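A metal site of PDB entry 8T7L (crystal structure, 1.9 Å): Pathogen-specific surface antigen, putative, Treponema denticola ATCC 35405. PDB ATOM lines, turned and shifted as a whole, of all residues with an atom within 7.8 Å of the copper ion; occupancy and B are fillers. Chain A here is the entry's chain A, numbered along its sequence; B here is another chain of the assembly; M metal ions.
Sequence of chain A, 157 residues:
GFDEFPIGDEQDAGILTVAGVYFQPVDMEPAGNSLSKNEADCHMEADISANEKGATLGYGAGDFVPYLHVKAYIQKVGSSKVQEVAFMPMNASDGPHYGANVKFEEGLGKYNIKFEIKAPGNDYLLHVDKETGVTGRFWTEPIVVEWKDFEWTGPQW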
ATOM      1  N   PHE A   2      -3.387  -6.056   9.925  1.00  0.00           N
ATOM      2  CA  PHE A   2      -4.578  -5.260  10.151  1.00  0.00           C
ATOM      3  C   PHE A   2      -4.420  -3.934   9.421  1.00  0.00           C
ATOM      4  O   PHE A   2      -3.304  -3.533   9.057  1.00  0.00           O
ATOM      5  CB  PHE A   2      -4.852  -5.081  11.667  1.00  0.00           C
ATOM      6  CG  PHE A   2      -3.779  -4.352  12.410  1.00  0.00           C
ATOM      7  CD1 PHE A   2      -3.704  -2.968  12.403  1.00  0.00           C
ATOM      8  CD2 PHE A   2      -2.816  -5.071  13.112  1.00  0.00           C
ATOM      9  CE1 PHE A   2      -2.701  -2.314  13.096  1.00  0.00           C
ATOM     10  CE2 PHE A   2      -1.813  -4.417  13.804  1.00  0.00           C
ATOM     11  CZ  PHE A   2      -1.752  -3.036  13.799  1.00  0.00           C
ATOM     12  N   PHE A  23      -5.546   3.564  13.665  1.00  0.00           N
ATOM     13  CA  PHE A  23      -6.434   2.478  13.286  1.00  0.00           C
ATOM     14  C   PHE A  23      -7.472   2.334  14.391  1.00  0.00           C
ATOM     15  O   PHE A  23      -7.540   3.174  15.293  1.00  0.00           O
ATOM     16  CB  PHE A  23      -5.658   1.194  12.982  1.00  0.00           C
ATOM     17  CG  PHE A  23      -4.568   0.873  13.965  1.00  0.00           C
ATOM     18  CD1 PHE A  23      -4.845   0.148  15.130  1.00  0.00           C
ATOM     19  CD2 PHE A  23      -3.258   1.273  13.732  1.00  0.00           C
ATOM     20  CE1 PHE A  23      -3.836  -0.186  16.029  1.00  0.00           C
ATOM     21  CE2 PHE A  23      -2.237   0.957  14.638  1.00  0.00           C
ATOM     22  CZ  PHE A  23      -2.538   0.228  15.784  1.00  0.00           C
ATOM     23  N   VAL A  26      -7.934  -0.055  20.526  1.00  0.00           N
ATOM     24  CA  VAL A  26      -7.468  -1.380  20.894  1.00  0.00           C
ATOM     25  C   VAL A  26      -7.628  -1.598  22.396  1.00  0.00           C
ATOM     26  O   VAL A  26      -7.804  -0.651  23.172  1.00  0.00           O
ATOM     27  CB  VAL A  26      -5.992  -1.596  20.484  1.00  0.00           C
ATOM     28  CG1 VAL A  26      -5.783  -1.274  18.983  1.00  0.00           C
ATOM     29  CG2 VAL A  26      -5.070  -0.763  21.373  1.00  0.00           C
ATOM     30  N   ASP A  27      -7.551  -2.865  22.800  1.00  0.00           N
ATOM     31  CA  ASP A  27      -7.515  -3.255  24.205  1.00  0.00           C
ATOM     32  C   ASP A  27      -6.063  -3.462  24.605  1.00  0.00           C
ATOM     33  O   ASP A  27      -5.336  -4.194  23.933  1.00  0.00           O
ATOM     34  CB  ASP A  27      -8.304  -4.553  24.442  1.00  0.00           C
ATOM     35  CG  ASP A  27      -9.811  -4.362  24.319  1.00  0.00           C
ATOM     36  OD1 ASP A  27     -10.352  -3.408  24.906  1.00  0.00           O
ATOM     37  OD2 ASP A  27     -10.455  -5.198  23.635  1.00  0.00           O
ATOM     38  N   MET A  28      -5.646  -2.844  25.711  1.00  0.00           N
ATOM     39  CA  MET A  28      -4.268  -2.902  26.143  1.00  0.00           C
ATOM     40  C   MET A  28      -4.211  -3.595  27.505  1.00  0.00           C
ATOM     41  O   MET A  28      -5.070  -3.341  28.359  1.00  0.00           O
ATOM     42  CB  MET A  28      -3.686  -1.494  26.244  1.00  0.00           C
ATOM     43  CG  MET A  28      -3.116  -0.980  24.926  1.00  0.00           C
ATOM     44  SD  MET A  28      -3.164   0.828  24.868  1.00  0.00           S
ATOM     45  CE  MET A  28      -4.909   1.190  25.113  1.00  0.00           C
ATOM     46  N   HIS A  43      -6.804   4.247  17.807  1.00  0.00           N
ATOM     47  CA  HIS A  43      -5.488   4.038  18.381  1.00  0.00           C
ATOM     48  C   HIS A  43      -4.503   4.779  17.489  1.00  0.00           C
ATOM     49  O   HIS A  43      -4.567   4.655  16.270  1.00  0.00           O
ATOM     50  CB  HIS A  43      -5.139   2.559  18.427  1.00  0.00           C
ATOM     51  CG  HIS A  43      -3.934   2.253  19.254  1.00  0.00           C
ATOM     52  ND1 HIS A  43      -3.921   2.433  20.620  1.00  0.00           N
ATOM     53  CD2 HIS A  43      -2.701   1.805  18.919  1.00  0.00           C
ATOM     54  CE1 HIS A  43      -2.738   2.079  21.099  1.00  0.00           C
ATOM     55  NE2 HIS A  43      -1.969   1.713  20.088  1.00  0.00           N
ATOM     56  N   MET A  44      -3.641   5.583  18.101  1.00  0.00           N
ATOM     57  CA  MET A  44      -2.645   6.335  17.365  1.00  0.00           C
ATOM     58  C   MET A  44      -1.277   5.797  17.753  1.00  0.00           C
ATOM     59  O   MET A  44      -1.021   5.524  18.931  1.00  0.00           O
ATOM     60  CB  MET A  44      -2.730   7.838  17.682  1.00  0.00           C
ATOM     61  CG  MET A  44      -1.880   8.721  16.796  1.00  0.00           C
ATOM     62  SD  MET A  44      -2.158  10.484  17.066  1.00  0.00           S
ATOM     63  CE  MET A  44      -3.710  10.712  16.186  1.00  0.00           C
ATOM     64  N   GLU A  45      -0.414   5.631  16.754  1.00  0.00           N
ATOM     65  CA  GLU A  45       0.871   4.991  16.950  1.00  0.00           C
ATOM     66  C   GLU A  45       1.976   5.872  16.370  1.00  0.00           C
ATOM     67  O   GLU A  45       1.807   6.455  15.288  1.00  0.00           O
ATOM     68  CB  GLU A  45       0.808   3.604  16.283  1.00  0.00           C
ATOM     69  CG  GLU A  45       2.083   2.898  15.970  1.00  0.00           C
ATOM     70  CD  GLU A  45       1.795   1.508  15.428  1.00  0.00           C
ATOM     71  OE1 GLU A  45       2.413   1.100  14.424  1.00  0.00           O
ATOM     72  OE2 GLU A  45       0.884   0.832  15.960  1.00  0.00           O
ATOM     73  N   ALA A  46       3.076   5.996  17.120  1.00  0.00           N
ATOM     74  CA  ALA A  46       4.318   6.556  16.615  1.00  0.00           C
ATOM     75  C   ALA A  46       5.307   5.419  16.410  1.00  0.00           C
ATOM     76  O   ALA A  46       5.682   4.738  17.379  1.00  0.00           O
ATOM     77  CB  ALA A  46       4.900   7.599  17.576  1.00  0.00           C
ATOM     78  N   MET A  88       2.511   5.346  25.345  1.00  0.00           N
ATOM     79  CA  MET A  88       3.325   4.408  26.083  1.00  0.00           C
ATOM     80  C   MET A  88       3.928   3.364  25.147  1.00  0.00           C
ATOM     81  O   MET A  88       3.356   3.086  24.081  1.00  0.00           O
ATOM     82  CB  MET A  88       2.508   3.701  27.185  1.00  0.00           C
ATOM     83  CG  MET A  88       2.161   4.633  28.350  1.00  0.00           C
ATOM     84  SD  MET A  88       1.143   3.848  29.623  1.00  0.00           S
ATOM     85  CE  MET A  88       2.386   2.870  30.476  1.00  0.00           C
ATOM     86  N   PRO A  89       5.072   2.793  25.504  1.00  0.00           N
ATOM     87  CA  PRO A  89       5.649   1.715  24.698  1.00  0.00           C
ATOM     88  C   PRO A  89       4.806   0.458  24.881  1.00  0.00           C
ATOM     89  O   PRO A  89       4.241   0.213  25.949  1.00  0.00           O
ATOM     90  CB  PRO A  89       7.053   1.519  25.295  1.00  0.00           C
ATOM     91  CG  PRO A  89       6.890   1.953  26.722  1.00  0.00           C
ATOM     92  CD  PRO A  89       5.907   3.085  26.692  1.00  0.00           C
ATOM     93  N   MET A  90       4.705  -0.322  23.808  1.00  0.00           N
ATOM     94  CA  MET A  90       3.828  -1.488  23.800  1.00  0.00           C
ATOM     95  C   MET A  90       4.101  -2.308  22.553  1.00  0.00           C
ATOM     96  O   MET A  90       4.706  -1.829  21.593  1.00  0.00           O
ATOM     97  CB  MET A  90       2.346  -1.093  23.829  1.00  0.00           C
ATOM     98  CG  MET A  90       1.905  -0.230  22.641  1.00  0.00           C
ATOM     99  SD  MET A  90       0.184   0.262  22.861  1.00  0.00           S
ATOM    100  CE  MET A  90       0.415   1.805  23.679  1.00  0.00           C
ATOM    101  N   ASN A  91       3.642  -3.568  22.592  1.00  0.00           N
ATOM    102  CA  ASN A  91       3.691  -4.465  21.455  1.00  0.00           C
ATOM    103  C   ASN A  91       2.286  -4.728  20.913  1.00  0.00           C
ATOM    104  O   ASN A  91       1.348  -4.970  21.679  1.00  0.00           O
ATOM    105  CB  ASN A  91       4.329  -5.815  21.857  1.00  0.00           C
ATOM    106  CG  ASN A  91       5.804  -5.891  21.519  1.00  0.00           C
ATOM    107  OD1 ASN A  91       6.438  -4.883  21.203  1.00  0.00           O
ATOM    108  ND2 ASN A  91       6.370  -7.087  21.607  1.00  0.00           N
ATOM    109  N   ALA A  92       2.156  -4.665  19.595  1.00  0.00           N
ATOM    110  CA  ALA A  92       1.009  -5.198  18.864  1.00  0.00           C
ATOM    111  C   ALA A  92       1.496  -6.394  18.051  1.00  0.00           C
ATOM    112  O   ALA A  92       2.674  -6.795  18.143  1.00  0.00           O
ATOM    113  CB  ALA A  92       0.390  -4.116  17.982  1.00  0.00           C
ATOM    114  N   ASP A  94       2.219  -6.424  15.098  1.00  0.00           N
ATOM    115  CA  ASP A  94       3.264  -5.936  14.201  1.00  0.00           C
ATOM    116  C   ASP A  94       4.489  -5.386  14.945  1.00  0.00           C
ATOM    117  O   ASP A  94       5.345  -4.754  14.317  1.00  0.00           O
ATOM    118  CB  ASP A  94       2.702  -4.844  13.275  1.00  0.00           C
ATOM    119  CG  ASP A  94       2.026  -3.713  14.038  1.00  0.00           C
ATOM    120  OD1 ASP A  94       2.303  -3.530  15.248  1.00  0.00           O
ATOM    121  OD2 ASP A  94       1.238  -2.980  13.409  1.00  0.00           O
ATOM    122  N   GLY A  95       4.586  -5.595  16.256  1.00  0.00           N
ATOM    123  CA  GLY A  95       5.805  -5.286  16.962  1.00  0.00           C
ATOM    124  C   GLY A  95       5.722  -4.072  17.860  1.00  0.00           C
ATOM    125  O   GLY A  95       4.645  -3.554  18.175  1.00  0.00           O
ATOM    126  N   PRO A  96       6.884  -3.585  18.303  1.00  0.00           N
ATOM    127  CA  PRO A  96       6.897  -2.506  19.293  1.00  0.00           C
ATOM    128  C   PRO A  96       6.595  -1.156  18.677  1.00  0.00           C
ATOM    129  O   PRO A  96       6.933  -0.868  17.523  1.00  0.00           O
ATOM    130  CB  PRO A  96       8.331  -2.536  19.864  1.00  0.00           C
ATOM    131  CG  PRO A  96       9.122  -3.406  18.948  1.00  0.00           C
ATOM    132  CD  PRO A  96       8.203  -4.164  18.050  1.00  0.00           C
ATOM    133  N   HIS A  97       5.969  -0.310  19.474  1.00  0.00           N
ATOM    134  CA  HIS A  97       5.706   1.058  19.065  1.00  0.00           C
ATOM    135  C   HIS A  97       5.368   1.848  20.312  1.00  0.00           C
ATOM    136  O   HIS A  97       5.229   1.299  21.398  1.00  0.00           O
ATOM    137  CB  HIS A  97       4.539   1.173  18.072  1.00  0.00           C
ATOM    138  CG  HIS A  97       3.234   0.584  18.552  1.00  0.00           C
ATOM    139  ND1 HIS A  97       2.938  -0.757  18.465  1.00  0.00           N
ATOM    140  CD2 HIS A  97       2.187   1.160  19.179  1.00  0.00           C
ATOM    141  CE1 HIS A  97       1.741  -0.979  18.972  1.00  0.00           C
ATOM    142  NE2 HIS A  97       1.252   0.166  19.416  1.00  0.00           N
ATOM    143  N   TYR A  98       5.218   3.151  20.132  1.00  0.00           N
ATOM    144  CA  TYR A  98       4.631   4.015  21.135  1.00  0.00           C
ATOM    145  C   TYR A  98       3.216   4.362  20.668  1.00  0.00           C
ATOM    146  O   TYR A  98       3.025   4.716  19.507  1.00  0.00           O
ATOM    147  CB  TYR A  98       5.449   5.286  21.331  1.00  0.00           C
ATOM    148  CG  TYR A  98       6.872   5.033  21.805  1.00  0.00           C
ATOM    149  CD1 TYR A  98       7.895   4.824  20.887  1.00  0.00           C
ATOM    150  CD2 TYR A  98       7.181   5.003  23.155  1.00  0.00           C
ATOM    151  CE1 TYR A  98       9.215   4.599  21.307  1.00  0.00           C
ATOM    152  CE2 TYR A  98       8.505   4.774  23.592  1.00  0.00           C
ATOM    153  CZ  TYR A  98       9.508   4.569  22.643  1.00  0.00           C
ATOM    154  OH  TYR A  98      10.816   4.346  23.024  1.00  0.00           O
ATOM    155  N   GLY A  99       2.248   4.268  21.572  1.00  0.00           N
ATOM    156  CA  GLY A  99       0.885   4.583  21.155  1.00  0.00           C
ATOM    157  C   GLY A  99      -0.046   4.932  22.295  1.00  0.00           C
ATOM    158  O   GLY A  99       0.325   4.915  23.469  1.00  0.00           O
ATOM    159  N   ALA A 100      -1.288   5.248  21.903  1.00  0.00           N
ATOM    160  CA  ALA A 100      -2.357   5.513  22.853  1.00  0.00           C
ATOM    161  C   ALA A 100      -3.680   5.434  22.100  1.00  0.00           C
ATOM    162  O   ALA A 100      -3.709   5.658  20.887  1.00  0.00           O
ATOM    163  CB  ALA A 100      -2.198   6.874  23.527  1.00  0.00           C
ATOM    164  N   ASN A 101      -4.759   5.110  22.821  1.00  0.00           N
ATOM    165  CA  ASN A 101      -6.091   5.313  22.273  1.00  0.00           C
ATOM    166  C   ASN A 101      -6.419   6.804  22.405  1.00  0.00           C
ATOM    167  O   ASN A 101      -6.206   7.391  23.471  1.00  0.00           O
ATOM    168  CB  ASN A 101      -7.115   4.476  23.039  1.00  0.00           C
ATOM    169  CG  ASN A 101      -7.085   3.003  22.642  1.00  0.00           C
ATOM    170  OD1 ASN A 101      -6.634   2.634  21.552  1.00  0.00           O
ATOM    171  ND2 ASN A 101      -7.628   2.147  23.512  1.00  0.00           N
ATOM    172  N   LEU B 125       3.053  -2.113  27.544  1.00  0.00           N
ATOM    173  CA  LEU B 125       1.718  -2.673  27.322  1.00  0.00           C
ATOM    174  C   LEU B 125       1.725  -3.712  26.223  1.00  0.00           C
ATOM    175  O   LEU B 125       2.673  -3.832  25.440  1.00  0.00           O
ATOM    176  CB  LEU B 125       0.725  -1.565  26.965  1.00  0.00           C
ATOM    177  CG  LEU B 125       0.694  -0.328  27.852  1.00  0.00           C
ATOM    178  CD1 LEU B 125      -0.536   0.536  27.591  1.00  0.00           C
ATOM    179  CD2 LEU B 125       0.822  -0.662  29.330  1.00  0.00           C
ATOM    180  N   LEU B 126       0.653  -4.504  26.174  1.00  0.00           N
ATOM    181  CA  LEU B 126       0.406  -5.453  25.093  1.00  0.00           C
ATOM    182  C   LEU B 126      -0.975  -5.185  24.519  1.00  0.00           C
ATOM    183  O   LEU B 126      -1.937  -5.079  25.278  1.00  0.00           O
ATOM    184  CB  LEU B 126       0.480  -6.887  25.613  1.00  0.00           C
ATOM    185  CG  LEU B 126       1.848  -7.467  25.981  1.00  0.00           C
ATOM    186  CD1 LEU B 126       1.681  -8.957  26.205  1.00  0.00           C
ATOM    187  CD2 LEU B 126       2.901  -7.224  24.888  1.00  0.00           C
ATOM    188  N   HIS B 127      -1.079  -5.054  23.187  1.00  0.00           N
ATOM    189  CA  HIS B 127      -2.383  -5.153  22.534  1.00  0.00           C
ATOM    190  C   HIS B 127      -2.912  -6.568  22.763  1.00  0.00           C
ATOM    191  O   HIS B 127      -2.204  -7.537  22.459  1.00  0.00           O
ATOM    192  CB  HIS B 127      -2.256  -4.887  21.037  1.00  0.00           C
ATOM    193  CG  HIS B 127      -1.979  -3.464  20.653  1.00  0.00           C
ATOM    194  ND1 HIS B 127      -2.564  -2.860  19.563  1.00  0.00           N
ATOM    195  CD2 HIS B 127      -1.134  -2.538  21.192  1.00  0.00           C
ATOM    196  CE1 HIS B 127      -2.095  -1.629  19.444  1.00  0.00           C
ATOM    197  NE2 HIS B 127      -1.221  -1.416  20.411  1.00  0.00           N
ATOM    198  N   THR B 132      -5.725  -6.640  16.511  1.00  0.00           N
ATOM    199  CA  THR B 132      -4.337  -6.156  16.455  1.00  0.00           C
ATOM    200  C   THR B 132      -3.433  -6.793  17.508  1.00  0.00           C
ATOM    201  O   THR B 132      -2.254  -6.420  17.606  1.00  0.00           O
ATOM    202  CB  THR B 132      -4.256  -4.634  16.673  1.00  0.00           C
ATOM    203  OG1 THR B 132      -4.528  -4.330  18.052  1.00  0.00           O
ATOM    204  CG2 THR B 132      -5.257  -3.884  15.799  1.00  0.00           C
HETATM  205 CU    CU M   1      -0.406   0.500  20.574  1.00  0.00          CU
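N of His 127 of chain B lies within hydrogen-bond range of O of Asn 91, at 2.9 Å. ND1 of His 43 is in hydrogen-bond range of O of Ala 100 (3.2 Å). O of Gly 95 lies within hydrogen-bond range of ND1 of His 97. The backbone carbonyl oxygen (O) of Phe 23 sits at hydrogen-bond distance from the backbone NH (N) of His 43 (2.8 Å). A ring nitrogen (ND1) of His 127 of chain B sits at hydrogen-bond distance from the side-chain hydroxyl of Thr 132 of chain B (2.9 Å). The side-chain amide oxygen (OD1) of Asn 101 is in hydrogen-bond range of a ring nitrogen (ND1) of His 43 (2.9 Å).
Within 4 Å of the copper ion: His 43, Met 90, His 97 and His 127 of chain B. The nearest printed residue that does not touch the copper ion is Gly 99 (4.3 Å).
The copper ion is bound by NE2 of His 43, NE2 of His 97, NE2 of His 127 of chain B and SD of Met 90. The copper ion has four donor atoms within binding distance.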
